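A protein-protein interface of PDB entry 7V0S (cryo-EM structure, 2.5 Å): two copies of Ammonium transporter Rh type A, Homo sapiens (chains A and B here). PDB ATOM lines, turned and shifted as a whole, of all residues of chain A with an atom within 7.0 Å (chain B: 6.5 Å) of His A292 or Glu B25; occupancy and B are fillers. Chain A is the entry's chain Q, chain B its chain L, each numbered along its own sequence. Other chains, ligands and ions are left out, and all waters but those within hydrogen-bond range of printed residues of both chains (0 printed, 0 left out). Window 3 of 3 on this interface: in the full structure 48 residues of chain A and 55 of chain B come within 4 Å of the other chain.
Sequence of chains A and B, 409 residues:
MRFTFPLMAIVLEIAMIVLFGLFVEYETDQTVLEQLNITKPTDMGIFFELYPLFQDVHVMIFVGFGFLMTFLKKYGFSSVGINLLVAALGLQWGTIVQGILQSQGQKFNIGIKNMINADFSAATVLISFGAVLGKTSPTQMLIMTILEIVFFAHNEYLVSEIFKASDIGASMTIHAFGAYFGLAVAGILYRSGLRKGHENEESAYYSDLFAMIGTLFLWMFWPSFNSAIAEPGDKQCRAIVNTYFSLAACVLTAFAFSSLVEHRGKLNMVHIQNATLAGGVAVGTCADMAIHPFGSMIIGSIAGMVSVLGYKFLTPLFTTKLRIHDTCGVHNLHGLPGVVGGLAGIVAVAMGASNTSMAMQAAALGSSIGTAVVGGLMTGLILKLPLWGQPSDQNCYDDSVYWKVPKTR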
ATOM      1  N   ARG A 238     -30.823  12.549  11.358  1.00  0.00           N
ATOM      2  CA  ARG A 238     -29.437  12.174  11.613  1.00  0.00           C
ATOM      3  C   ARG A 238     -28.506  13.361  11.420  1.00  0.00           C
ATOM      4  O   ARG A 238     -27.578  13.560  12.209  1.00  0.00           O
ATOM      5  CB  ARG A 238     -29.030  11.015  10.705  1.00  0.00           C
ATOM      6  CG  ARG A 238     -29.333   9.642  11.277  1.00  0.00           C
ATOM      7  CD  ARG A 238     -28.364   8.594  10.761  1.00  0.00           C
ATOM      8  NE  ARG A 238     -28.337   8.529   9.306  1.00  0.00           N
ATOM      9  CZ  ARG A 238     -29.143   7.774   8.573  1.00  0.00           C
ATOM     10  NH1 ARG A 238     -30.063   7.003   9.129  1.00  0.00           N
ATOM     11  NH2 ARG A 238     -29.023   7.794   7.249  1.00  0.00           N
ATOM     12  N   VAL A 241     -28.960  15.720  14.510  1.00  0.00           N
ATOM     13  CA  VAL A 241     -28.358  15.182  15.730  1.00  0.00           C
ATOM     14  C   VAL A 241     -26.834  15.187  15.633  1.00  0.00           C
ATOM     15  O   VAL A 241     -26.135  15.560  16.591  1.00  0.00           O
ATOM     16  CB  VAL A 241     -28.913  13.772  16.010  1.00  0.00           C
ATOM     17  CG1 VAL A 241     -28.174  13.114  17.159  1.00  0.00           C
ATOM     18  CG2 VAL A 241     -30.398  13.842  16.315  1.00  0.00           C
ATOM     19  N   ASN A 242     -26.297  14.783  14.479  1.00  0.00           N
ATOM     20  CA  ASN A 242     -24.853  14.726  14.295  1.00  0.00           C
ATOM     21  C   ASN A 242     -24.227  16.111  14.388  1.00  0.00           C
ATOM     22  O   ASN A 242     -23.203  16.291  15.056  1.00  0.00           O
ATOM     23  CB  ASN A 242     -24.528  14.075  12.952  1.00  0.00           C
ATOM     24  CG  ASN A 242     -24.674  12.568  12.988  1.00  0.00           C
ATOM     25  OD1 ASN A 242     -24.526  11.945  14.036  1.00  0.00           O
ATOM     26  ND2 ASN A 242     -24.965  11.974  11.838  1.00  0.00           N
ATOM     27  N   CYS A 286     -20.397  13.795   6.578  1.00  0.00           N
ATOM     28  CA  CYS A 286     -20.931  12.648   7.301  1.00  0.00           C
ATOM     29  C   CYS A 286     -22.221  12.951   8.049  1.00  0.00           C
ATOM     30  O   CYS A 286     -22.646  12.125   8.864  1.00  0.00           O
ATOM     31  CB  CYS A 286     -19.900  12.125   8.305  1.00  0.00           C
ATOM     32  SG  CYS A 286     -18.393  11.486   7.590  1.00  0.00           S
ATOM     33  N   MET A 289     -25.106  10.586   7.212  1.00  0.00           N
ATOM     34  CA  MET A 289     -24.663   9.177   7.269  1.00  0.00           C
ATOM     35  C   MET A 289     -24.881   8.655   8.688  1.00  0.00           C
ATOM     36  O   MET A 289     -24.948   9.469   9.597  1.00  0.00           O
ATOM     37  CB  MET A 289     -23.189   9.064   6.873  1.00  0.00           C
ATOM     38  CG  MET A 289     -22.857   9.654   5.519  1.00  0.00           C
ATOM     39  SD  MET A 289     -21.116   9.341   5.152  1.00  0.00           S
ATOM     40  CE  MET A 289     -20.833  10.417   3.748  1.00  0.00           C
ATOM     41  N   ALA A 290     -25.020   7.340   8.852  1.00  0.00           N
ATOM     42  CA  ALA A 290     -25.188   6.744  10.198  1.00  0.00           C
ATOM     43  C   ALA A 290     -23.828   6.492  10.854  1.00  0.00           C
ATOM     44  O   ALA A 290     -23.413   5.338  10.915  1.00  0.00           O
ATOM     45  CB  ALA A 290     -26.022   5.496  10.093  1.00  0.00           C
ATOM     46  N   ILE A 291     -23.155   7.555  11.290  1.00  0.00           N
ATOM     47  CA  ILE A 291     -21.832   7.442  11.958  1.00  0.00           C
ATOM     48  C   ILE A 291     -22.052   7.250  13.450  1.00  0.00           C
ATOM     49  O   ILE A 291     -21.067   6.948  14.121  1.00  0.00           O
ATOM     50  CB  ILE A 291     -21.004   8.698  11.646  1.00  0.00           C
ATOM     51  CG1 ILE A 291     -21.656   9.951  12.239  1.00  0.00           C
ATOM     52  CG2 ILE A 291     -20.783   8.837  10.149  1.00  0.00           C
ATOM     53  CD1 ILE A 291     -20.959  11.239  11.891  1.00  0.00           C
ATOM     54  N   HIS A 292     -23.275   7.468  13.929  1.00  0.00           N
ATOM     55  CA  HIS A 292     -23.625   7.405  15.374  1.00  0.00           C
ATOM     56  C   HIS A 292     -23.381   8.814  15.951  1.00  0.00           C
ATOM     57  O   HIS A 292     -22.533   9.521  15.417  1.00  0.00           O
ATOM     58  CB  HIS A 292     -22.931   6.242  16.098  1.00  0.00           C
ATOM     59  CG  HIS A 292     -23.343   6.031  17.510  1.00  0.00           C
ATOM     60  ND1 HIS A 292     -22.955   6.877  18.525  1.00  0.00           N
ATOM     61  CD2 HIS A 292     -24.083   5.063  18.085  1.00  0.00           C
ATOM     62  CE1 HIS A 292     -23.450   6.452  19.666  1.00  0.00           C
ATOM     63  NE2 HIS A 292     -24.133   5.339  19.421  1.00  0.00           N
ATOM     64  N   PRO A 293     -24.035   9.232  17.044  1.00  0.00           N
ATOM     65  CA  PRO A 293     -23.734  10.507  17.691  1.00  0.00           C
ATOM     66  C   PRO A 293     -22.284  10.517  18.219  1.00  0.00           C
ATOM     67  O   PRO A 293     -21.658  11.532  18.151  1.00  0.00           O
ATOM     68  CB  PRO A 293     -24.828  10.632  18.765  1.00  0.00           C
ATOM     69  CG  PRO A 293     -25.946   9.767  18.253  1.00  0.00           C
ATOM     70  CD  PRO A 293     -25.239   8.604  17.599  1.00  0.00           C
ATOM     71  N   PHE A 294     -21.806   9.401  18.749  1.00  0.00           N
ATOM     72  CA  PHE A 294     -20.431   9.314  19.302  1.00  0.00           C
ATOM     73  C   PHE A 294     -19.394   9.568  18.206  1.00  0.00           C
ATOM     74  O   PHE A 294     -18.407  10.261  18.503  1.00  0.00           O
ATOM     75  CB  PHE A 294     -20.224   7.975  20.014  1.00  0.00           C
ATOM     76  CG  PHE A 294     -19.425   6.936  19.283  1.00  0.00           C
ATOM     77  CD1 PHE A 294     -18.043   6.999  19.242  1.00  0.00           C
ATOM     78  CD2 PHE A 294     -20.056   5.871  18.670  1.00  0.00           C
ATOM     79  CE1 PHE A 294     -17.312   6.038  18.567  1.00  0.00           C
ATOM     80  CE2 PHE A 294     -19.321   4.906  18.005  1.00  0.00           C
ATOM     81  CZ  PHE A 294     -17.952   4.992  17.954  1.00  0.00           C
ATOM     82  N   GLY A 295     -19.604   9.040  16.999  1.00  0.00           N
ATOM     83  CA  GLY A 295     -18.699   9.320  15.872  1.00  0.00           C
ATOM     84  C   GLY A 295     -18.709  10.792  15.515  1.00  0.00           C
ATOM     85  O   GLY A 295     -17.646  11.344  15.275  1.00  0.00           O
ATOM     86  N   SER A 296     -19.876  11.410  15.543  1.00  0.00           N
ATOM     87  CA  SER A 296     -20.004  12.859  15.275  1.00  0.00           C
ATOM     88  C   SER A 296     -19.221  13.639  16.336  1.00  0.00           C
ATOM     89  O   SER A 296     -18.570  14.608  15.975  1.00  0.00           O
ATOM     90  CB  SER A 296     -21.457  13.235  15.201  1.00  0.00           C
ATOM     91  OG  SER A 296     -22.029  13.334  16.489  1.00  0.00           O
ATOM     92  N   MET A 297     -19.276  13.211  17.585  1.00  0.00           N
ATOM     93  CA  MET A 297     -18.506  13.854  18.679  1.00  0.00           C
ATOM     94  C   MET A 297     -16.988  13.732  18.473  1.00  0.00           C
ATOM     95  O   MET A 297     -16.293  14.692  18.780  1.00  0.00           O
ATOM     96  CB  MET A 297     -18.934  13.281  20.022  1.00  0.00           C
ATOM     97  CG  MET A 297     -20.241  13.847  20.505  1.00  0.00           C
ATOM     98  SD  MET A 297     -21.008  12.741  21.698  1.00  0.00           S
ATOM     99  CE  MET A 297     -20.224  13.284  23.212  1.00  0.00           C
ATOM    100  N   ALA A 353     -20.919   2.962   6.479  1.00  0.00           N
ATOM    101  CA  ALA A 353     -21.959   3.903   6.953  1.00  0.00           C
ATOM    102  C   ALA A 353     -22.711   4.438   5.740  1.00  0.00           C
ATOM    103  O   ALA A 353     -23.910   4.743   5.871  1.00  0.00           O
ATOM    104  CB  ALA A 353     -21.330   5.013   7.743  1.00  0.00           C
ATOM    105  N   ILE B  17     -17.863  11.125  25.025  1.00  0.00           N
ATOM    106  CA  ILE B  17     -17.817  10.302  23.818  1.00  0.00           C
ATOM    107  C   ILE B  17     -18.040   8.835  24.166  1.00  0.00           C
ATOM    108  O   ILE B  17     -18.818   8.132  23.509  1.00  0.00           O
ATOM    109  CB  ILE B  17     -16.481  10.511  23.082  1.00  0.00           C
ATOM    110  CG1 ILE B  17     -16.420  11.904  22.455  1.00  0.00           C
ATOM    111  CG2 ILE B  17     -16.273   9.441  22.021  1.00  0.00           C
ATOM    112  CD1 ILE B  17     -15.030  12.320  22.054  1.00  0.00           C
ATOM    113  N   PHE B  20     -21.700   8.236  25.220  1.00  0.00           N
ATOM    114  CA  PHE B  20     -22.568   8.224  24.048  1.00  0.00           C
ATOM    115  C   PHE B  20     -22.414   6.929  23.261  1.00  0.00           C
ATOM    116  O   PHE B  20     -23.402   6.367  22.779  1.00  0.00           O
ATOM    117  CB  PHE B  20     -22.270   9.428  23.159  1.00  0.00           C
ATOM    118  CG  PHE B  20     -23.180  10.591  23.396  1.00  0.00           C
ATOM    119  CD1 PHE B  20     -23.095  11.322  24.568  1.00  0.00           C
ATOM    120  CD2 PHE B  20     -24.117  10.957  22.449  1.00  0.00           C
ATOM    121  CE1 PHE B  20     -23.927  12.393  24.789  1.00  0.00           C
ATOM    122  CE2 PHE B  20     -24.954  12.030  22.668  1.00  0.00           C
ATOM    123  CZ  PHE B  20     -24.857  12.745  23.841  1.00  0.00           C
ATOM    124  N   GLY B  21     -21.181   6.443  23.115  1.00  0.00           N
ATOM    125  CA  GLY B  21     -20.979   5.169  22.448  1.00  0.00           C
ATOM    126  C   GLY B  21     -21.620   4.010  23.184  1.00  0.00           C
ATOM    127  O   GLY B  21     -22.103   3.063  22.561  1.00  0.00           O
ATOM    128  N   LEU B  22     -21.636   4.070  24.515  1.00  0.00           N
ATOM    129  CA  LEU B  22     -22.198   2.987  25.314  1.00  0.00           C
ATOM    130  C   LEU B  22     -23.722   3.015  25.380  1.00  0.00           C
ATOM    131  O   LEU B  22     -24.347   1.952  25.425  1.00  0.00           O
ATOM    132  CB  LEU B  22     -21.621   3.033  26.729  1.00  0.00           C
ATOM    133  CG  LEU B  22     -20.169   2.583  26.891  1.00  0.00           C
ATOM    134  CD1 LEU B  22     -19.673   2.879  28.292  1.00  0.00           C
ATOM    135  CD2 LEU B  22     -20.031   1.107  26.572  1.00  0.00           C
ATOM    136  N   PHE B  23     -24.342   4.198  25.392  1.00  0.00           N
ATOM    137  CA  PHE B  23     -25.753   4.304  25.745  1.00  0.00           C
ATOM    138  C   PHE B  23     -26.666   4.857  24.660  1.00  0.00           C
ATOM    139  O   PHE B  23     -27.885   4.704  24.778  1.00  0.00           O
ATOM    140  CB  PHE B  23     -25.920   5.182  26.995  1.00  0.00           C
ATOM    141  CG  PHE B  23     -25.445   4.536  28.260  1.00  0.00           C
ATOM    142  CD1 PHE B  23     -26.135   3.471  28.809  1.00  0.00           C
ATOM    143  CD2 PHE B  23     -24.307   4.993  28.899  1.00  0.00           C
ATOM    144  CE1 PHE B  23     -25.702   2.877  29.973  1.00  0.00           C
ATOM    145  CE2 PHE B  23     -23.869   4.403  30.062  1.00  0.00           C
ATOM    146  CZ  PHE B  23     -24.567   3.344  30.601  1.00  0.00           C
ATOM    147  N   VAL B  24     -26.132   5.480  23.617  1.00  0.00           N
ATOM    148  CA  VAL B  24     -26.927   6.324  22.733  1.00  0.00           C
ATOM    149  C   VAL B  24     -27.098   5.651  21.378  1.00  0.00           C
ATOM    150  O   VAL B  24     -26.165   5.055  20.834  1.00  0.00           O
ATOM    151  CB  VAL B  24     -26.275   7.720  22.589  1.00  0.00           C
ATOM    152  CG1 VAL B  24     -26.857   8.487  21.419  1.00  0.00           C
ATOM    153  CG2 VAL B  24     -26.426   8.505  23.878  1.00  0.00           C
ATOM    154  N   GLU B  25     -28.322   5.717  20.855  1.00  0.00           N
ATOM    155  CA  GLU B  25     -28.625   5.326  19.485  1.00  0.00           C
ATOM    156  C   GLU B  25     -29.506   6.395  18.852  1.00  0.00           C
ATOM    157  O   GLU B  25     -30.051   7.261  19.537  1.00  0.00           O
ATOM    158  CB  GLU B  25     -29.325   3.960  19.410  1.00  0.00           C
ATOM    159  CG  GLU B  25     -28.685   2.867  20.247  1.00  0.00           C
ATOM    160  CD  GLU B  25     -27.508   2.214  19.547  1.00  0.00           C
ATOM    161  OE1 GLU B  25     -26.918   1.276  20.123  1.00  0.00           O
ATOM    162  OE2 GLU B  25     -27.176   2.629  18.417  1.00  0.00           O
ATOM    163  N   TYR B  26     -29.625   6.337  17.529  1.00  0.00           N
ATOM    164  CA  TYR B  26     -30.503   7.257  16.810  1.00  0.00           C
ATOM    165  C   TYR B  26     -31.967   6.968  17.119  1.00  0.00           C
ATOM    166  O   TYR B  26     -32.841   7.790  16.847  1.00  0.00           O
ATOM    167  CB  TYR B  26     -30.270   7.173  15.300  1.00  0.00           C
ATOM    168  CG  TYR B  26     -28.983   7.806  14.832  1.00  0.00           C
ATOM    169  CD1 TYR B  26     -28.772   9.171  14.963  1.00  0.00           C
ATOM    170  CD2 TYR B  26     -27.987   7.040  14.245  1.00  0.00           C
ATOM    171  CE1 TYR B  26     -27.599   9.755  14.531  1.00  0.00           C
ATOM    172  CE2 TYR B  26     -26.812   7.613  13.811  1.00  0.00           C
ATOM    173  CZ  TYR B  26     -26.624   8.970  13.953  1.00  0.00           C
ATOM    174  OH  TYR B  26     -25.454   9.542  13.519  1.00  0.00           O
ATOM    175  N   LYS B 107     -30.016   1.183  26.943  1.00  0.00           N
ATOM    176  CA  LYS B 107     -29.767   2.045  25.799  1.00  0.00           C
ATOM    177  C   LYS B 107     -31.034   2.809  25.434  1.00  0.00           C
ATOM    178  O   LYS B 107     -32.155   2.323  25.597  1.00  0.00           O
ATOM    179  CB  LYS B 107     -29.290   1.225  24.601  1.00  0.00           C
ATOM    180  CG  LYS B 107     -27.847   0.790  24.682  1.00  0.00           C
ATOM    181  CD  LYS B 107     -27.212   0.742  23.306  1.00  0.00           C
ATOM    182  CE  LYS B 107     -25.907  -0.030  23.335  1.00  0.00           C
ATOM    183  NZ  LYS B 107     -24.748   0.823  22.961  1.00  0.00           N
ATOM    184  N   PHE B 108     -30.848   4.025  24.931  1.00  0.00           N
ATOM    185  CA  PHE B 108     -31.978   4.870  24.587  1.00  0.00           C
ATOM    186  C   PHE B 108     -31.689   5.593  23.281  1.00  0.00           C
ATOM    187  O   PHE B 108     -30.534   5.793  22.900  1.00  0.00           O
ATOM    188  CB  PHE B 108     -32.298   5.866  25.714  1.00  0.00           C
ATOM    189  CG  PHE B 108     -31.188   6.836  26.013  1.00  0.00           C
ATOM    190  CD1 PHE B 108     -30.191   6.508  26.914  1.00  0.00           C
ATOM    191  CD2 PHE B 108     -31.155   8.084  25.408  1.00  0.00           C
ATOM    192  CE1 PHE B 108     -29.172   7.397  27.196  1.00  0.00           C
ATOM    193  CE2 PHE B 108     -30.140   8.976  25.686  1.00  0.00           C
ATOM    194  CZ  PHE B 108     -29.146   8.632  26.581  1.00  0.00           C
ATOM    195  N   ASN B 109     -32.760   5.978  22.599  1.00  0.00           N
ATOM    196  CA  ASN B 109     -32.684   6.692  21.335  1.00  0.00           C
ATOM    197  C   ASN B 109     -32.782   8.193  21.571  1.00  0.00           C
ATOM    198  O   ASN B 109     -33.258   8.652  22.611  1.00  0.00           O
ATOM    199  CB  ASN B 109     -33.792   6.229  20.389  1.00  0.00           C
ATOM    200  CG  ASN B 109     -34.030   4.735  20.464  1.00  0.00           C
ATOM    201  OD1 ASN B 109     -33.170   3.940  20.091  1.00  0.00           O
ATOM    202  ND2 ASN B 109     -35.201   4.346  20.949  1.00  0.00           N
ATOM    203  N   ILE B 110     -32.317   8.960  20.591  1.00  0.00           N
ATOM    204  CA  ILE B 110     -32.255  10.413  20.697  1.00  0.00           C
ATOM    205  C   ILE B 110     -33.192  11.017  19.664  1.00  0.00           C
ATOM    206  O   ILE B 110     -33.030  10.802  18.456  1.00  0.00           O
ATOM    207  CB  ILE B 110     -30.827  10.945  20.522  1.00  0.00           C
ATOM    208  CG1 ILE B 110     -29.986  10.595  21.749  1.00  0.00           C
ATOM    209  CG2 ILE B 110     -30.849  12.451  20.273  1.00  0.00           C
ATOM    210  CD1 ILE B 110     -28.771  11.457  21.914  1.00  0.00           C
ATOM    211  N   GLY B 111     -34.171  11.783  20.142  1.00  0.00           N
ATOM    212  CA  GLY B 111     -35.033  12.568  19.297  1.00  0.00           C
ATOM    213  C   GLY B 111     -34.900  14.053  19.575  1.00  0.00           C
ATOM    214  O   GLY B 111     -33.939  14.522  20.185  1.00  0.00           O
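O of Val B24 lies within hydrogen-bond range of NE2 of His A292, at 2.5 Å.
The side-chain hydroxyl (OH) of Tyr B26 is in hydrogen-bond range of the backbone NH (N) of His A292, 3.0 Å away.
The side-chain hydroxyl of Tyr B26 lies within hydrogen-bond range of the side-chain amide oxygen of Asn A242, 2.6 Å away.
The backbone NH of Glu B25 is in hydrogen-bond range of the backbone carbonyl oxygen of Phe B108, at 3.0 Å.
O of Met A289 lies within hydrogen-bond range of ND2 of Asn A242, at 3.4 Å.
The backbone carbonyl oxygen (O) of Arg A238 sits at hydrogen-bond distance from the side-chain amide nitrogen (ND2) of Asn A242 (3.1 Å).
N of Phe A294 is in hydrogen-bond range of ND1 of His A292, 2.8 Å away.
The backbone NH of Ile B110 is in hydrogen-bond range of the backbone carbonyl oxygen of Glu B25 (3.0 Å).
The backbone carbonyl oxygen (O) of Asn A242 is in hydrogen-bond range of the side-chain hydroxyl (OG) of Ser A296 (3.5 Å).
Arg A238 touches Tyr B26 (CD to CE2, 3.6 Å).
Met A289 touches Tyr B26 (O to OH, 3.96 Å).
His A292 touches Phe B20 (CE1 to O, 3.1 Å).
CA of Gly B21 touches CE1 of His A292, at 3.9 Å.
His A292 touches Glu B25 (CD2 to OE2, 3.9 Å).
Tyr B26 touches Pro A293 (OH to N, 3.8 Å).
Phe A294 touches Ile B17.
Gly B21 touches Phe A294 (N to CB, 3.6 Å).
Met A297 touches Ile B17.
SD of Met A297 touches CG of Phe B20 (3.5 Å).
His A292 touches five residues of chain B.
Printed residues of chain B within 4 Å of Pro A293: Phe B20 (3.8 Å), Val B24 (3.5 Å) and Tyr B26 (3.8 Å).
Of the printed residues of chain B, Phe A294 touches Ile B17 (3.8 Å) and Gly B21 (3.6 Å).
Printed residues of chain A within 4 Å of Val B24: His A292 and Pro A293.
Phe B108 touches none of the printed residues of chain A.
The nearest residue of chain A that does not touch Glu B25 is Pro A293 (4.9 Å).
The nearest printed residue of chain B that does not touch Met A289 is Glu B25 (10.8 Å).
Of the 14 printed residues of chain A, 8 touch a printed residue of chain B.
Hydrophobic or aromatic side chains of chain A within 4 Å of the printed part of chain B: His A292, Pro A293, Phe A294 and Met A297.
Of the 13 printed residues of chain B, 6 touch a printed residue of chain A.
Hydrophobic or aromatic side chains of chain B that line the printed part of chain A: Ile B17, Phe B20, Val B24 and Tyr B26.
Among the printed residues, no Asp or Glu carboxylate lies within 4 Å of a Lys or Arg side-chain nitrogen of the other chain.
No position is printed for both chains.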
